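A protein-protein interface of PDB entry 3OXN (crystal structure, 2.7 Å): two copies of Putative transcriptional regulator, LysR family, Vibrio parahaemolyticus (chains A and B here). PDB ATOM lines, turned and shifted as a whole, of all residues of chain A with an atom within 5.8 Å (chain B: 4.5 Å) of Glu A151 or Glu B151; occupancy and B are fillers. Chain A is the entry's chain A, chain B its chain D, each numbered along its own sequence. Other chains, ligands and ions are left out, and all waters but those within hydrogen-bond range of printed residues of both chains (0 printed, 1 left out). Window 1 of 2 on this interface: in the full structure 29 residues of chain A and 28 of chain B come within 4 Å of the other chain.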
ATOM      1  N   MET A  30      -3.600  15.645 -32.191  1.00  0.00           N
ATOM      2  CA  MET A  30      -2.801  16.160 -31.098  1.00  0.00           C
ATOM      3  C   MET A  30      -2.946  15.300 -29.868  1.00  0.00           C
ATOM      4  O   MET A  30      -2.207  15.451 -28.897  1.00  0.00           O
ATOM      5  CB  MET A  30      -3.243  17.589 -30.779  1.00  0.00           C
ATOM      6  CG  MET A  30      -2.155  18.412 -30.166  1.00  0.00           C
ATOM      7  SD  MET A  30      -0.548  18.337 -31.284  1.00  0.00           S
ATOM      8  CE  MET A  30       0.774  18.290 -29.836  1.00  0.00           C
ATOM      9  N   GLN A  31      -3.915  14.396 -29.916  1.00  0.00           N
ATOM     10  CA  GLN A  31      -4.224  13.523 -28.790  1.00  0.00           C
ATOM     11  C   GLN A  31      -3.959  12.048 -29.097  1.00  0.00           C
ATOM     12  O   GLN A  31      -3.797  11.241 -28.182  1.00  0.00           O
ATOM     13  CB  GLN A  31      -5.689  13.705 -28.386  1.00  0.00           C
ATOM     14  CG  GLN A  31      -5.943  14.883 -27.461  1.00  0.00           C
ATOM     15  CD  GLN A  31      -7.411  15.277 -27.403  1.00  0.00           C
ATOM     16  OE1 GLN A  31      -7.829  16.036 -26.523  1.00  0.00           O
ATOM     17  NE2 GLN A  31      -8.201  14.771 -28.349  1.00  0.00           N
ATOM     18  N   PRO A  35       1.238  12.321 -29.777  1.00  0.00           N
ATOM     19  CA  PRO A  35       1.663  11.720 -28.507  1.00  0.00           C
ATOM     20  C   PRO A  35       2.297  10.353 -28.771  1.00  0.00           C
ATOM     21  O   PRO A  35       3.365  10.021 -28.255  1.00  0.00           O
ATOM     22  CB  PRO A  35       0.349  11.568 -27.741  1.00  0.00           C
ATOM     23  CG  PRO A  35      -0.507  12.678 -28.256  1.00  0.00           C
ATOM     24  CD  PRO A  35      -0.115  12.902 -29.701  1.00  0.00           C
ATOM     25  N   HIS A 149     -11.520  20.032 -27.460  1.00  0.00           N
ATOM     26  CA  HIS A 149     -10.951  19.172 -26.433  1.00  0.00           C
ATOM     27  C   HIS A 149     -12.169  18.428 -25.931  1.00  0.00           C
ATOM     28  O   HIS A 149     -13.276  18.962 -25.988  1.00  0.00           O
ATOM     29  CB  HIS A 149     -10.302  19.974 -25.306  1.00  0.00           C
ATOM     30  CG  HIS A 149      -9.300  20.985 -25.785  1.00  0.00           C
ATOM     31  ND1 HIS A 149      -8.183  20.644 -26.507  1.00  0.00           N
ATOM     32  CD2 HIS A 149      -9.255  22.336 -25.632  1.00  0.00           C
ATOM     33  CE1 HIS A 149      -7.493  21.740 -26.796  1.00  0.00           C
ATOM     34  NE2 HIS A 149      -8.120  22.773 -26.273  1.00  0.00           N
ATOM     35  N   LEU A 150     -11.997  17.193 -25.478  1.00  0.00           N
ATOM     36  CA  LEU A 150     -13.151  16.442 -25.001  1.00  0.00           C
ATOM     37  C   LEU A 150     -13.457  16.578 -23.507  1.00  0.00           C
ATOM     38  O   LEU A 150     -14.496  16.093 -23.057  1.00  0.00           O
ATOM     39  CB  LEU A 150     -13.089  14.960 -25.397  1.00  0.00           C
ATOM     40  CG  LEU A 150     -11.907  14.025 -25.097  1.00  0.00           C
ATOM     41  CD1 LEU A 150     -10.902  14.520 -24.029  1.00  0.00           C
ATOM     42  CD2 LEU A 150     -12.508  12.683 -24.708  1.00  0.00           C
ATOM     43  N   GLU A 151     -12.588  17.224 -22.734  1.00  0.00           N
ATOM     44  CA  GLU A 151     -12.901  17.439 -21.319  1.00  0.00           C
ATOM     45  C   GLU A 151     -14.180  18.254 -21.120  1.00  0.00           C
ATOM     46  O   GLU A 151     -14.629  18.442 -19.996  1.00  0.00           O
ATOM     47  CB  GLU A 151     -11.738  18.074 -20.561  1.00  0.00           C
ATOM     48  CG  GLU A 151     -10.649  18.634 -21.458  1.00  0.00           C
ATOM     49  CD  GLU A 151      -9.344  17.835 -21.388  1.00  0.00           C
ATOM     50  OE1 GLU A 151      -8.851  17.573 -20.256  1.00  0.00           O
ATOM     51  OE2 GLU A 151      -8.814  17.489 -22.474  1.00  0.00           O
ATOM     52  N   ALA A 152     -14.771  18.723 -22.213  1.00  0.00           N
ATOM     53  CA  ALA A 152     -16.038  19.452 -22.143  1.00  0.00           C
ATOM     54  C   ALA A 152     -17.216  18.485 -22.195  1.00  0.00           C
ATOM     55  O   ALA A 152     -18.149  18.592 -21.406  1.00  0.00           O
ATOM     56  CB  ALA A 152     -16.143  20.494 -23.269  1.00  0.00           C
ATOM     57  N   ALA A 153     -17.175  17.542 -23.134  1.00  0.00           N
ATOM     58  CA  ALA A 153     -18.190  16.496 -23.175  1.00  0.00           C
ATOM     59  C   ALA A 153     -18.097  15.665 -21.896  1.00  0.00           C
ATOM     60  O   ALA A 153     -19.115  15.391 -21.265  1.00  0.00           O
ATOM     61  CB  ALA A 153     -18.035  15.628 -24.408  1.00  0.00           C
ATOM     62  N   LEU A 154     -16.877  15.287 -21.507  1.00  0.00           N
ATOM     63  CA  LEU A 154     -16.659  14.588 -20.243  1.00  0.00           C
ATOM     64  C   LEU A 154     -17.503  15.266 -19.175  1.00  0.00           C
ATOM     65  O   LEU A 154     -18.267  14.612 -18.468  1.00  0.00           O
ATOM     66  CB  LEU A 154     -15.178  14.606 -19.825  1.00  0.00           C
ATOM     67  CG  LEU A 154     -14.120  13.909 -20.700  1.00  0.00           C
ATOM     68  CD1 LEU A 154     -12.702  14.007 -20.110  1.00  0.00           C
ATOM     69  CD2 LEU A 154     -14.477  12.445 -20.971  1.00  0.00           C
ATOM     70  N   ALA A 155     -17.385  16.590 -19.087  1.00  0.00           N
ATOM     71  CA  ALA A 155     -18.064  17.377 -18.065  1.00  0.00           C
ATOM     72  C   ALA A 155     -19.552  17.090 -17.951  1.00  0.00           C
ATOM     73  O   ALA A 155     -20.123  17.226 -16.877  1.00  0.00           O
ATOM     74  CB  ALA A 155     -17.837  18.854 -18.310  1.00  0.00           C
ATOM     75  N   TYR A 178     -11.655   6.615 -19.062  1.00  0.00           N
ATOM     76  CA  TYR A 178     -12.684   7.443 -18.458  1.00  0.00           C
ATOM     77  C   TYR A 178     -13.885   6.559 -18.200  1.00  0.00           C
ATOM     78  O   TYR A 178     -15.023   7.027 -18.114  1.00  0.00           O
ATOM     79  CB  TYR A 178     -13.054   8.603 -19.377  1.00  0.00           C
ATOM     80  CG  TYR A 178     -12.004   9.677 -19.446  1.00  0.00           C
ATOM     81  CD1 TYR A 178     -11.843  10.583 -18.404  1.00  0.00           C
ATOM     82  CD2 TYR A 178     -11.173   9.787 -20.548  1.00  0.00           C
ATOM     83  CE1 TYR A 178     -10.878  11.578 -18.463  1.00  0.00           C
ATOM     84  CE2 TYR A 178     -10.205  10.771 -20.619  1.00  0.00           C
ATOM     85  CZ  TYR A 178     -10.061  11.667 -19.575  1.00  0.00           C
ATOM     86  OH  TYR A 178      -9.099  12.651 -19.643  1.00  0.00           O
ATOM     87  N   GLN B  31     -10.212  23.685 -21.526  1.00  0.00           N
ATOM     88  CA  GLN B  31      -9.945  22.540 -20.662  1.00  0.00           C
ATOM     89  C   GLN B  31     -10.239  22.812 -19.194  1.00  0.00           C
ATOM     90  O   GLN B  31     -10.415  21.881 -18.402  1.00  0.00           O
ATOM     91  CB  GLN B  31      -8.499  22.062 -20.833  1.00  0.00           C
ATOM     92  CG  GLN B  31      -8.039  22.044 -22.284  1.00  0.00           C
ATOM     93  CD  GLN B  31      -6.559  21.755 -22.426  1.00  0.00           C
ATOM     94  OE1 GLN B  31      -6.094  20.668 -22.061  1.00  0.00           O
ATOM     95  NE2 GLN B  31      -5.809  22.719 -22.972  1.00  0.00           N
ATOM     96  N   PRO B  35     -15.467  23.659 -19.141  1.00  0.00           N
ATOM     97  CA  PRO B  35     -15.965  22.378 -18.630  1.00  0.00           C
ATOM     98  C   PRO B  35     -16.393  22.499 -17.188  1.00  0.00           C
ATOM     99  O   PRO B  35     -17.313  21.818 -16.762  1.00  0.00           O
ATOM    100  CB  PRO B  35     -14.753  21.464 -18.732  1.00  0.00           C
ATOM    101  CG  PRO B  35     -13.899  22.088 -19.763  1.00  0.00           C
ATOM    102  CD  PRO B  35     -14.085  23.560 -19.627  1.00  0.00           C
ATOM    103  N   HIS B 149      -1.941  20.766 -25.542  1.00  0.00           N
ATOM    104  CA  HIS B 149      -2.561  19.558 -25.032  1.00  0.00           C
ATOM    105  C   HIS B 149      -1.498  18.835 -24.241  1.00  0.00           C
ATOM    106  O   HIS B 149      -0.520  18.361 -24.815  1.00  0.00           O
ATOM    107  CB  HIS B 149      -2.990  18.670 -26.190  1.00  0.00           C
ATOM    108  CG  HIS B 149      -3.839  19.367 -27.198  1.00  0.00           C
ATOM    109  ND1 HIS B 149      -5.147  19.003 -27.447  1.00  0.00           N
ATOM    110  CD2 HIS B 149      -3.577  20.418 -28.011  1.00  0.00           C
ATOM    111  CE1 HIS B 149      -5.647  19.797 -28.379  1.00  0.00           C
ATOM    112  NE2 HIS B 149      -4.721  20.671 -28.732  1.00  0.00           N
ATOM    113  N   LEU B 150      -1.657  18.744 -22.928  1.00  0.00           N
ATOM    114  CA  LEU B 150      -0.609  18.107 -22.149  1.00  0.00           C
ATOM    115  C   LEU B 150      -0.586  16.596 -22.407  1.00  0.00           C
ATOM    116  O   LEU B 150       0.306  15.886 -21.936  1.00  0.00           O
ATOM    117  CB  LEU B 150      -0.738  18.427 -20.663  1.00  0.00           C
ATOM    118  CG  LEU B 150      -1.864  17.748 -19.887  1.00  0.00           C
ATOM    119  CD1 LEU B 150      -1.599  17.927 -18.397  1.00  0.00           C
ATOM    120  CD2 LEU B 150      -3.253  18.290 -20.290  1.00  0.00           C
ATOM    121  N   GLU B 151      -1.565  16.110 -23.166  1.00  0.00           N
ATOM    122  CA  GLU B 151      -1.533  14.731 -23.629  1.00  0.00           C
ATOM    123  C   GLU B 151      -0.164  14.564 -24.257  1.00  0.00           C
ATOM    124  O   GLU B 151       0.503  13.560 -24.053  1.00  0.00           O
ATOM    125  CB  GLU B 151      -2.616  14.488 -24.682  1.00  0.00           C
ATOM    126  CG  GLU B 151      -3.655  15.624 -24.811  1.00  0.00           C
ATOM    127  CD  GLU B 151      -4.847  15.487 -23.860  1.00  0.00           C
ATOM    128  OE1 GLU B 151      -5.594  14.483 -23.967  1.00  0.00           O
ATOM    129  OE2 GLU B 151      -5.045  16.397 -23.022  1.00  0.00           O
ATOM    130  N   ALA B 152       0.257  15.594 -24.991  1.00  0.00           N
ATOM    131  CA  ALA B 152       1.524  15.612 -25.730  1.00  0.00           C
ATOM    132  C   ALA B 152       2.752  15.718 -24.844  1.00  0.00           C
ATOM    133  O   ALA B 152       3.784  15.123 -25.146  1.00  0.00           O
ATOM    134  CB  ALA B 152       1.528  16.741 -26.752  1.00  0.00           C
ATOM    135  N   ALA B 153       2.673  16.494 -23.768  1.00  0.00           N
ATOM    136  CA  ALA B 153       3.797  16.534 -22.830  1.00  0.00           C
ATOM    137  C   ALA B 153       3.898  15.214 -22.046  1.00  0.00           C
ATOM    138  O   ALA B 153       4.991  14.706 -21.789  1.00  0.00           O
ATOM    139  CB  ALA B 153       3.683  17.716 -21.894  1.00  0.00           C
ATOM    140  N   LEU B 154       2.745  14.662 -21.682  1.00  0.00           N
ATOM    141  CA  LEU B 154       2.684  13.406 -20.967  1.00  0.00           C
ATOM    142  C   LEU B 154       3.453  12.408 -21.768  1.00  0.00           C
ATOM    143  O   LEU B 154       4.274  11.672 -21.239  1.00  0.00           O
ATOM    144  CB  LEU B 154       1.243  12.935 -20.861  1.00  0.00           C
ATOM    145  CG  LEU B 154       0.394  13.777 -19.916  1.00  0.00           C
ATOM    146  CD1 LEU B 154      -1.084  13.575 -20.231  1.00  0.00           C
ATOM    147  CD2 LEU B 154       0.717  13.447 -18.462  1.00  0.00           C
ATOM    148  N   ALA B 155       3.189  12.404 -23.064  1.00  0.00           N
ATOM    149  CA  ALA B 155       3.831  11.468 -23.976  1.00  0.00           C
ATOM    150  C   ALA B 155       5.358  11.379 -23.800  1.00  0.00           C
ATOM    151  O   ALA B 155       5.950  10.347 -24.118  1.00  0.00           O
ATOM    152  CB  ALA B 155       3.466  11.806 -25.422  1.00  0.00           C
ATOM    153  N   TYR B 178      -3.475  12.280 -13.885  1.00  0.00           N
ATOM    154  CA  TYR B 178      -2.473  11.685 -14.752  1.00  0.00           C
ATOM    155  C   TYR B 178      -1.306  11.267 -13.887  1.00  0.00           C
ATOM    156  O   TYR B 178      -0.241  10.895 -14.381  1.00  0.00           O
ATOM    157  CB  TYR B 178      -1.990  12.656 -15.812  1.00  0.00           C
ATOM    158  CG  TYR B 178      -2.987  12.983 -16.895  1.00  0.00           C
ATOM    159  CD1 TYR B 178      -3.398  12.025 -17.814  1.00  0.00           C
ATOM    160  CD2 TYR B 178      -3.486  14.267 -17.024  1.00  0.00           C
ATOM    161  CE1 TYR B 178      -4.297  12.346 -18.815  1.00  0.00           C
ATOM    162  CE2 TYR B 178      -4.374  14.595 -18.007  1.00  0.00           C
ATOM    163  CZ  TYR B 178      -4.778  13.640 -18.901  1.00  0.00           C
ATOM    164  OH  TYR B 178      -5.673  13.999 -19.882  1.00  0.00           O
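Of the printed residues of chain B, Glu A151 touches Pro B35 and Glu B151. Ala A152 touches none of the printed residues of chain B. Ala A153 touches none of the printed residues of chain B. Printed residues of chain B within 4 Å of Ala A155: Pro B35. Printed residues of chain A within 4 Å of His B149: Met A30 and His A149. Glu B151 touches two residues of chain A.
His B149 touches Met A30. Ala B152 touches Met A30. CG of Gln A31 touches OE1 of Glu B151, at 3.5 Å. O of Pro A35 touches CB of Ala B155, at 3.3 Å. His A149 touches Gln B31. His A149 touches His B149 (CE1 to CE1, 3.1 Å). Glu A151 touches Pro B35. OE2 of Glu B151 touches OE2 of Glu A151, 3.96 Å away. Pro B35 touches Ala A155. OH of Tyr A178 touches OH of Tyr B178, 3.7 Å away.
Pro A35 touches Ala B155, and with the chains exchanged Ala A155 touches Pro B35. His A149 touches Gln B31, but with the chains exchanged Gln A31 does not touch His B149 (4.1 Å). His A149 touches its own counterpart, His B149. Tyr A178 touches its own counterpart, Tyr B178. Positions printed for both chains: 31, 35, 149, 150, 151, 152, 153, 154, 155 and 178.
Of the 11 printed residues of chain A, 7 touch a printed residue of chain B. Hydrophobic or aromatic side chains of chain A that line the printed part of chain B: Met A30, Pro A35, His A149, Ala A155 and Tyr A178. Of the 10 printed residues of chain B, 7 touch a printed residue of chain A. Hydrophobic or aromatic side chains of chain B within 4 Å of the printed part of chain A: Pro B35, His B149, Ala B152, Ala B155 and Tyr B178.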
